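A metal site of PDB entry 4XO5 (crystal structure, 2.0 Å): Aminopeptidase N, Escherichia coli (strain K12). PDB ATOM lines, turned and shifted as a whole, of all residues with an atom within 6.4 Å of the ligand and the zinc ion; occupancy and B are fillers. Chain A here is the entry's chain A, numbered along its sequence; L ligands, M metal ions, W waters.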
ATOM      1  N   GLN A 115       0.279  -0.542 -11.078  1.00  0.00           N
ATOM      2  CA  GLN A 115      -0.429  -1.000 -12.270  1.00  0.00           C
ATOM      3  C   GLN A 115      -0.489   0.176 -13.245  1.00  0.00           C
ATOM      4  O   GLN A 115      -1.092   1.226 -12.910  1.00  0.00           O
ATOM      5  CB  GLN A 115      -1.841  -1.518 -11.929  1.00  0.00           C
ATOM      6  CG  GLN A 115      -2.706  -1.842 -13.153  1.00  0.00           C
ATOM      7  CD  GLN A 115      -2.012  -2.891 -14.040  1.00  0.00           C
ATOM      8  OE1 GLN A 115      -1.351  -3.779 -13.535  1.00  0.00           O
ATOM      9  NE2 GLN A 115      -2.207  -2.802 -15.369  1.00  0.00           N
ATOM     10  N   CYS A 116       0.186   0.039 -14.386  1.00  0.00           N
ATOM     11  CA  CYS A 116       0.312   1.108 -15.348  1.00  0.00           C
ATOM     12  C   CYS A 116      -0.511   0.944 -16.619  1.00  0.00           C
ATOM     13  O   CYS A 116      -0.731   1.919 -17.302  1.00  0.00           O
ATOM     14  CB  CYS A 116       1.775   1.371 -15.697  1.00  0.00           C
ATOM     15  SG  CYS A 116       2.740   1.944 -14.256  1.00  0.00           S
ATOM     16  N   GLU A 117      -0.928  -0.267 -16.959  1.00  0.00           N
ATOM     17  CA  GLU A 117      -1.765  -0.418 -18.152  1.00  0.00           C
ATOM     18  C   GLU A 117      -3.198  -0.022 -17.783  1.00  0.00           C
ATOM     19  O   GLU A 117      -3.699  -0.501 -16.781  1.00  0.00           O
ATOM     20  CB  GLU A 117      -1.728  -1.843 -18.719  1.00  0.00           C
ATOM     21  CG  GLU A 117      -2.397  -1.925 -20.088  1.00  0.00           C
ATOM     22  CD  GLU A 117      -2.441  -3.320 -20.712  1.00  0.00           C
ATOM     23  OE1 GLU A 117      -1.880  -4.229 -20.087  1.00  0.00           O
ATOM     24  OE2 GLU A 117      -2.918  -3.448 -21.848  1.00  0.00           O
ATOM     25  N   ALA A 118      -3.913   0.735 -18.645  1.00  0.00           N
ATOM     26  CA  ALA A 118      -3.412   1.299 -19.911  1.00  0.00           C
ATOM     27  C   ALA A 118      -2.674   2.617 -19.702  1.00  0.00           C
ATOM     28  O   ALA A 118      -1.628   2.837 -20.346  1.00  0.00           O
ATOM     29  CB  ALA A 118      -4.579   1.591 -20.870  1.00  0.00           C
ATOM     30  N   TYR A 181       3.480   1.662 -20.146  1.00  0.00           N
ATOM     31  CA  TYR A 181       2.464   0.762 -19.509  1.00  0.00           C
ATOM     32  C   TYR A 181       3.083  -0.531 -18.978  1.00  0.00           C
ATOM     33  O   TYR A 181       2.453  -1.199 -18.156  1.00  0.00           O
ATOM     34  CB  TYR A 181       1.271   0.438 -20.400  1.00  0.00           C
ATOM     35  CG  TYR A 181       1.479  -0.584 -21.491  1.00  0.00           C
ATOM     36  CD1 TYR A 181       1.238  -1.934 -21.230  1.00  0.00           C
ATOM     37  CD2 TYR A 181       1.860  -0.223 -22.806  1.00  0.00           C
ATOM     38  CE1 TYR A 181       1.411  -2.885 -22.211  1.00  0.00           C
ATOM     39  CE2 TYR A 181       2.019  -1.196 -23.805  1.00  0.00           C
ATOM     40  CZ  TYR A 181       1.840  -2.537 -23.471  1.00  0.00           C
ATOM     41  OH  TYR A 181       2.013  -3.518 -24.398  1.00  0.00           O
ATOM     42  N   PHE A 254      -5.874  -6.049  -6.537  1.00  0.00           N
ATOM     43  CA  PHE A 254      -5.550  -5.889  -7.954  1.00  0.00           C
ATOM     44  C   PHE A 254      -6.849  -5.876  -8.722  1.00  0.00           C
ATOM     45  O   PHE A 254      -7.680  -6.735  -8.485  1.00  0.00           O
ATOM     46  CB  PHE A 254      -4.665  -7.070  -8.370  1.00  0.00           C
ATOM     47  CG  PHE A 254      -3.907  -6.846  -9.640  1.00  0.00           C
ATOM     48  CD1 PHE A 254      -2.811  -5.984  -9.651  1.00  0.00           C
ATOM     49  CD2 PHE A 254      -4.322  -7.475 -10.835  1.00  0.00           C
ATOM     50  CE1 PHE A 254      -2.103  -5.773 -10.796  1.00  0.00           C
ATOM     51  CE2 PHE A 254      -3.645  -7.203 -12.033  1.00  0.00           C
ATOM     52  CZ  PHE A 254      -2.516  -6.388 -12.011  1.00  0.00           C
ATOM     53  N   MET A 256      -7.520  -6.376 -12.013  1.00  0.00           N
ATOM     54  CA  MET A 256      -7.665  -7.375 -13.114  1.00  0.00           C
ATOM     55  C   MET A 256      -7.133  -8.741 -12.646  1.00  0.00           C
ATOM     56  O   MET A 256      -7.139  -9.072 -11.425  1.00  0.00           O
ATOM     57  CB  MET A 256      -6.911  -6.843 -14.319  1.00  0.00           C
ATOM     58  CG  MET A 256      -7.278  -5.379 -14.668  1.00  0.00           C
ATOM     59  SD  MET A 256      -8.976  -5.284 -15.286  1.00  0.00           S
ATOM     60  CE  MET A 256      -9.021  -6.374 -16.741  1.00  0.00           C
ATOM     61  N   GLY A 257      -6.694  -9.532 -13.588  1.00  0.00           N
ATOM     62  CA  GLY A 257      -6.193 -10.825 -13.333  1.00  0.00           C
ATOM     63  C   GLY A 257      -4.703 -10.758 -13.118  1.00  0.00           C
ATOM     64  O   GLY A 257      -4.200 -11.269 -12.137  1.00  0.00           O
ATOM     65  N   ALA A 258      -3.984 -10.245 -14.100  1.00  0.00           N
ATOM     66  CA  ALA A 258      -2.549 -10.200 -13.942  1.00  0.00           C
ATOM     67  C   ALA A 258      -1.955  -9.246 -14.975  1.00  0.00           C
ATOM     68  O   ALA A 258      -2.660  -8.794 -15.870  1.00  0.00           O
ATOM     69  CB  ALA A 258      -1.940 -11.586 -14.047  1.00  0.00           C
ATOM     70  N   MET A 259      -0.688  -8.987 -14.913  1.00  0.00           N
ATOM     71  CA  MET A 259      -0.099  -7.973 -15.796  1.00  0.00           C
ATOM     72  C   MET A 259       1.287  -8.363 -16.257  1.00  0.00           C
ATOM     73  O   MET A 259       2.155  -8.724 -15.443  1.00  0.00           O
ATOM     74  CB  MET A 259      -0.054  -6.648 -15.108  1.00  0.00           C
ATOM     75  CG  MET A 259       0.570  -5.523 -15.906  1.00  0.00           C
ATOM     76  SD  MET A 259      -0.440  -5.146 -17.375  1.00  0.00           S
ATOM     77  CE  MET A 259       0.862  -4.597 -18.488  1.00  0.00           C
ATOM     78  N   GLU A 260       1.513  -8.231 -17.549  1.00  0.00           N
ATOM     79  CA  GLU A 260       2.775  -8.707 -18.185  1.00  0.00           C
ATOM     80  C   GLU A 260       3.988  -7.762 -18.143  1.00  0.00           C
ATOM     81  O   GLU A 260       4.828  -7.783 -19.060  1.00  0.00           O
ATOM     82  CB  GLU A 260       2.461  -9.054 -19.631  1.00  0.00           C
ATOM     83  CG  GLU A 260       2.207  -7.841 -20.576  1.00  0.00           C
ATOM     84  CD  GLU A 260       0.698  -7.436 -20.730  1.00  0.00           C
ATOM     85  OE1 GLU A 260      -0.142  -7.758 -19.857  1.00  0.00           O
ATOM     86  OE2 GLU A 260       0.375  -6.799 -21.769  1.00  0.00           O
ATOM     87  N   HIS A 293      -0.656 -16.972 -20.185  1.00  0.00           N
ATOM     88  CA  HIS A 293      -1.042 -15.725 -20.866  1.00  0.00           C
ATOM     89  C   HIS A 293      -0.013 -14.617 -20.651  1.00  0.00           C
ATOM     90  O   HIS A 293       0.462 -14.007 -21.606  1.00  0.00           O
ATOM     91  CB  HIS A 293      -2.445 -15.285 -20.295  1.00  0.00           C
ATOM     92  CG  HIS A 293      -3.019 -14.073 -20.936  1.00  0.00           C
ATOM     93  ND1 HIS A 293      -3.883 -14.126 -21.988  1.00  0.00           N
ATOM     94  CD2 HIS A 293      -2.788 -12.764 -20.720  1.00  0.00           C
ATOM     95  CE1 HIS A 293      -4.144 -12.912 -22.417  1.00  0.00           C
ATOM     96  NE2 HIS A 293      -3.462 -12.074 -21.684  1.00  0.00           N
ATOM     97  N   GLU A 294       0.326 -14.330 -19.406  1.00  0.00           N
ATOM     98  CA  GLU A 294       1.256 -13.230 -19.140  1.00  0.00           C
ATOM     99  C   GLU A 294       2.651 -13.531 -19.719  1.00  0.00           C
ATOM    100  O   GLU A 294       3.312 -12.662 -20.246  1.00  0.00           O
ATOM    101  CB  GLU A 294       1.307 -12.893 -17.676  1.00  0.00           C
ATOM    102  CG  GLU A 294      -0.027 -12.596 -16.977  1.00  0.00           C
ATOM    103  CD  GLU A 294      -0.939 -11.581 -17.697  1.00  0.00           C
ATOM    104  OE1 GLU A 294      -0.432 -10.750 -18.382  1.00  0.00           O
ATOM    105  OE2 GLU A 294      -2.158 -11.710 -17.590  1.00  0.00           O
ATOM    106  N   HIS A 297       2.708 -12.942 -23.465  1.00  0.00           N
ATOM    107  CA  HIS A 297       2.811 -11.546 -23.784  1.00  0.00           C
ATOM    108  C   HIS A 297       4.275 -11.101 -23.938  1.00  0.00           C
ATOM    109  O   HIS A 297       4.529 -10.064 -24.509  1.00  0.00           O
ATOM    110  CB  HIS A 297       2.187 -10.660 -22.695  1.00  0.00           C
ATOM    111  CG  HIS A 297       0.735 -10.318 -22.900  1.00  0.00           C
ATOM    112  ND1 HIS A 297       0.228  -9.777 -24.074  1.00  0.00           N
ATOM    113  CD2 HIS A 297      -0.307 -10.363 -22.007  1.00  0.00           C
ATOM    114  CE1 HIS A 297      -1.060  -9.531 -23.912  1.00  0.00           C
ATOM    115  NE2 HIS A 297      -1.404  -9.903 -22.676  1.00  0.00           N
ATOM    116  N   LEU A 312      -5.468  -2.659 -29.090  1.00  0.00           N
ATOM    117  CA  LEU A 312      -5.356  -3.561 -27.974  1.00  0.00           C
ATOM    118  C   LEU A 312      -5.499  -5.058 -28.345  1.00  0.00           C
ATOM    119  O   LEU A 312      -4.700  -5.900 -27.870  1.00  0.00           O
ATOM    120  CB  LEU A 312      -6.334  -3.215 -26.884  1.00  0.00           C
ATOM    121  CG  LEU A 312      -6.361  -4.097 -25.646  1.00  0.00           C
ATOM    122  CD1 LEU A 312      -5.008  -4.018 -24.909  1.00  0.00           C
ATOM    123  CD2 LEU A 312      -7.420  -3.641 -24.632  1.00  0.00           C
ATOM    124  N   LYS A 315      -2.439  -7.438 -29.259  1.00  0.00           N
ATOM    125  CA  LYS A 315      -1.772  -8.224 -28.262  1.00  0.00           C
ATOM    126  C   LYS A 315      -2.764  -9.073 -27.501  1.00  0.00           C
ATOM    127  O   LYS A 315      -2.437 -10.212 -27.139  1.00  0.00           O
ATOM    128  CB  LYS A 315      -0.887  -7.381 -27.333  1.00  0.00           C
ATOM    129  CG  LYS A 315      -1.599  -6.501 -26.304  1.00  0.00           C
ATOM    130  CD  LYS A 315      -0.597  -5.631 -25.508  1.00  0.00           C
ATOM    131  CE  LYS A 315      -1.220  -4.745 -24.420  1.00  0.00           C
ATOM    132  NZ  LYS A 315      -1.728  -5.413 -23.183  1.00  0.00           N
ATOM    133  N   GLU A 316      -3.992  -8.594 -27.284  1.00  0.00           N
ATOM    134  CA  GLU A 316      -4.887  -9.401 -26.435  1.00  0.00           C
ATOM    135  C   GLU A 316      -5.547 -10.562 -27.172  1.00  0.00           C
ATOM    136  O   GLU A 316      -5.596 -11.686 -26.622  1.00  0.00           O
ATOM    137  CB  GLU A 316      -5.896  -8.625 -25.650  1.00  0.00           C
ATOM    138  CG  GLU A 316      -5.326  -7.596 -24.700  1.00  0.00           C
ATOM    139  CD  GLU A 316      -4.381  -8.212 -23.691  1.00  0.00           C
ATOM    140  OE1 GLU A 316      -4.487  -9.440 -23.487  1.00  0.00           O
ATOM    141  OE2 GLU A 316      -3.565  -7.476 -23.110  1.00  0.00           O
ATOM    142  N   THR A 319      -2.663 -13.112 -27.724  1.00  0.00           N
ATOM    143  CA  THR A 319      -2.195 -13.732 -26.496  1.00  0.00           C
ATOM    144  C   THR A 319      -3.237 -14.675 -25.897  1.00  0.00           C
ATOM    145  O   THR A 319      -2.890 -15.710 -25.347  1.00  0.00           O
ATOM    146  CB  THR A 319      -1.678 -12.695 -25.519  1.00  0.00           C
ATOM    147  OG1 THR A 319      -0.676 -11.898 -26.181  1.00  0.00           O
ATOM    148  CG2 THR A 319      -1.085 -13.362 -24.301  1.00  0.00           C
ATOM    149  N   VAL A 320      -4.519 -14.289 -25.981  1.00  0.00           N
ATOM    150  CA  VAL A 320      -5.580 -15.197 -25.583  1.00  0.00           C
ATOM    151  C   VAL A 320      -5.591 -16.435 -26.492  1.00  0.00           C
ATOM    152  O   VAL A 320      -5.733 -17.567 -25.986  1.00  0.00           O
ATOM    153  CB  VAL A 320      -6.960 -14.542 -25.641  1.00  0.00           C
ATOM    154  CG1 VAL A 320      -8.034 -15.626 -25.420  1.00  0.00           C
ATOM    155  CG2 VAL A 320      -7.117 -13.491 -24.570  1.00  0.00           C
ATOM    156  N   ASN A 369      -9.878   1.988 -20.114  1.00  0.00           N
ATOM    157  CA  ASN A 369     -10.026   0.850 -19.268  1.00  0.00           C
ATOM    158  C   ASN A 369     -11.360   0.184 -19.442  1.00  0.00           C
ATOM    159  O   ASN A 369     -11.472  -0.956 -19.052  1.00  0.00           O
ATOM    160  CB  ASN A 369      -9.799   1.092 -17.765  1.00  0.00           C
ATOM    161  CG  ASN A 369      -8.331   1.441 -17.446  1.00  0.00           C
ATOM    162  OD1 ASN A 369      -7.377   0.842 -17.988  1.00  0.00           O
ATOM    163  ND2 ASN A 369      -8.169   2.483 -16.609  1.00  0.00           N
ATOM    164  N   TYR A 372     -11.152  -3.367 -22.027  1.00  0.00           N
ATOM    165  CA  TYR A 372     -10.561  -4.673 -21.704  1.00  0.00           C
ATOM    166  C   TYR A 372     -11.694  -5.692 -21.637  1.00  0.00           C
ATOM    167  O   TYR A 372     -12.088  -6.148 -20.544  1.00  0.00           O
ATOM    168  CB  TYR A 372      -9.727  -4.548 -20.378  1.00  0.00           C
ATOM    169  CG  TYR A 372      -8.457  -3.785 -20.706  1.00  0.00           C
ATOM    170  CD1 TYR A 372      -8.463  -2.399 -20.905  1.00  0.00           C
ATOM    171  CD2 TYR A 372      -7.271  -4.463 -20.932  1.00  0.00           C
ATOM    172  CE1 TYR A 372      -7.343  -1.729 -21.325  1.00  0.00           C
ATOM    173  CE2 TYR A 372      -6.113  -3.805 -21.341  1.00  0.00           C
ATOM    174  CZ  TYR A 372      -6.134  -2.434 -21.497  1.00  0.00           C
ATOM    175  OH  TYR A 372      -4.997  -1.817 -21.937  1.00  0.00           O
ATOM    176  N   TYR A 377     -10.785  -9.396 -26.126  1.00  0.00           N
ATOM    177  CA  TYR A 377     -10.069 -10.622 -25.689  1.00  0.00           C
ATOM    178  C   TYR A 377     -10.568 -11.883 -26.440  1.00  0.00           C
ATOM    179  O   TYR A 377      -9.820 -12.509 -27.178  1.00  0.00           O
ATOM    180  CB  TYR A 377     -10.166 -10.841 -24.168  1.00  0.00           C
ATOM    181  CG  TYR A 377      -9.207 -10.003 -23.381  1.00  0.00           C
ATOM    182  CD1 TYR A 377      -9.328  -8.614 -23.385  1.00  0.00           C
ATOM    183  CD2 TYR A 377      -8.189 -10.600 -22.630  1.00  0.00           C
ATOM    184  CE1 TYR A 377      -8.424  -7.817 -22.672  1.00  0.00           C
ATOM    185  CE2 TYR A 377      -7.274  -9.833 -21.867  1.00  0.00           C
ATOM    186  CZ  TYR A 377      -7.393  -8.463 -21.863  1.00  0.00           C
ATOM    187  OH  TYR A 377      -6.502  -7.657 -21.198  1.00  0.00           O
ATOM    188  N   GLN A 817     -12.755   1.583 -11.879  1.00  0.00           N
ATOM    189  CA  GLN A 817     -12.617   0.441 -12.787  1.00  0.00           C
ATOM    190  C   GLN A 817     -13.482  -0.731 -12.334  1.00  0.00           C
ATOM    191  O   GLN A 817     -14.117  -1.356 -13.121  1.00  0.00           O
ATOM    192  CB  GLN A 817     -11.178  -0.085 -12.847  1.00  0.00           C
ATOM    193  CG  GLN A 817     -10.344   0.858 -13.630  1.00  0.00           C
ATOM    194  CD  GLN A 817      -8.920   0.272 -13.790  1.00  0.00           C
ATOM    195  OE1 GLN A 817      -8.681  -0.924 -14.202  1.00  0.00           O
ATOM    196  NE2 GLN A 817      -7.999   1.085 -13.466  1.00  0.00           N
ATOM    197  N   ARG A 821     -16.961  -2.435 -14.207  1.00  0.00           N
ATOM    198  CA  ARG A 821     -17.237  -3.867 -14.458  1.00  0.00           C
ATOM    199  C   ARG A 821     -18.598  -4.282 -13.869  1.00  0.00           C
ATOM    200  O   ARG A 821     -19.323  -4.998 -14.476  1.00  0.00           O
ATOM    201  CB  ARG A 821     -16.117  -4.766 -13.872  1.00  0.00           C
ATOM    202  CG  ARG A 821     -14.747  -4.469 -14.479  1.00  0.00           C
ATOM    203  CD  ARG A 821     -13.927  -5.681 -14.967  1.00  0.00           C
ATOM    204  NE  ARG A 821     -14.155  -5.876 -16.418  1.00  0.00           N
ATOM    205  CZ  ARG A 821     -13.265  -5.758 -17.427  1.00  0.00           C
ATOM    206  NH1 ARG A 821     -13.697  -5.930 -18.642  1.00  0.00           N
ATOM    207  NH2 ARG A 821     -11.972  -5.486 -17.297  1.00  0.00           N
HETATM  208  N1  LIG L   1      -2.629  -6.720 -20.254  1.00  0.00           N
HETATM  209  C1  LIG L   1      -3.136  -7.553 -19.082  1.00  0.00           C
HETATM  210  C2  LIG L   1      -3.540  -8.934 -19.618  1.00  0.00           C
HETATM  211  O1  LIG L   1      -2.950  -9.897 -19.275  1.00  0.00           O
HETATM  212  C3  LIG L   1      -4.353  -6.908 -18.359  1.00  0.00           C
HETATM  213  C4  LIG L   1      -4.061  -5.519 -17.735  1.00  0.00           C
HETATM  214  C5  LIG L   1      -5.261  -4.576 -17.697  1.00  0.00           C
HETATM  215  O2  LIG L   1      -6.440  -4.999 -17.633  1.00  0.00           O
HETATM  216  O3  LIG L   1      -5.012  -3.391 -17.654  1.00  0.00           O
HETATM  217  O4  LIG L   1      -4.455  -9.102 -20.385  1.00  0.00           O
HETATM  218 ZN    ZN M   1      -3.327 -10.068 -21.970  1.00  0.00          ZN
HETATM  219  O   HOH W   1      -7.201  -1.817 -17.698  1.00  0.00           O
HETATM  220  O   HOH W   2      -5.850  -9.443 -16.487  1.00  0.00           O
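O2 of the ligand lies close to SD of Met 256 (3.5 Å).
Residues that only touch the ligand: Tyr 372 (3.4 Å), Ala 258 (3.5 Å), Met 259 (3.7 Å) and Gln 115 (3.7 Å).
Hydrophobic or aromatic side chains that line the ligand: Met 256, Met 259, His 293, His 297, Tyr 372 and Tyr 377.
13 residues have an atom within 4 Å of the ligand: Gln 115, Glu 117, Met 256, Ala 258, Met 259, Glu 260, His 293, Glu 294, His 297, Lys 315, Glu 316, Tyr 372 and Tyr 377.
The nearest printed residue that does not touch the ligand is Ala 118 (4.4 Å).
OE2 of Glu 316 lies within salt-bridge range of NZ of Lys 315 (2.8 Å).
OE2 of Glu 260 is in salt-bridge range of NZ of Lys 315, 2.9 Å away.
The backbone carbonyl oxygen (O) of Tyr 372 is in hydrogen-bond range of the guanidinium group (NH1) of Arg 821, 2.5 Å away.
The side-chain sulfur of Met 256 sits close to the guanidinium group of Arg 821, 3.6 Å away.
The side-chain carboxylate (OE1) of Glu 294 lies within hydrogen-bond range of the backbone NH (N) of Glu 260 (3.3 Å).
The side-chain carboxylate (OE2) of Glu 117 is in hydrogen-bond range of the side-chain hydroxyl (OH) of Tyr 372, 2.6 Å away.
ND1 of His 297 is in hydrogen-bond range of OG1 of Thr 319 (3.1 Å).
The side-chain amide nitrogen of Gln 115 lies within hydrogen-bond range of the backbone carbonyl oxygen of Glu 117.
Merely in contact with the zinc ion: Tyr 377.
The nearest printed residue that does not touch the zinc ion is Glu 260 (4.5 Å).
The zinc ion is bound by OE1 of Glu 316.
The zinc ion is bound by NE2 of His 293 (2.0 Å).
The zinc ion is bound by a ring nitrogen (NE2) of His 297.
O4 of the ligand is bound to the zinc ion.
Slightly farther from the zinc ion lies O1 of the ligand (2.7 Å).
Slightly farther from the zinc ion lies the side-chain carboxylate (OE2) of Glu 316 (2.8 Å).
Water W1 lies within hydrogen-bond range of the side-chain amide oxygen of Asn 369 and an oxygen (O3) of the ligand.
OE1 of Glu 117 is in salt-bridge range of N1 of the ligand (2.6 Å).
NZ of Lys 315 lies close to N1 of the ligand, at 3.3 Å.
The side-chain carboxylate (OE2) of Glu 294 sits close to an oxygen (O1) of the ligand, 2.6 Å away.
The side-chain hydroxyl (OH) of Tyr 377 lies close to an oxygen (O4) of the ligand, at 2.6 Å.
A nitrogen (N1) of the ligand lies within salt-bridge range of the side-chain carboxylate (OE1) of Glu 260 (2.7 Å).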
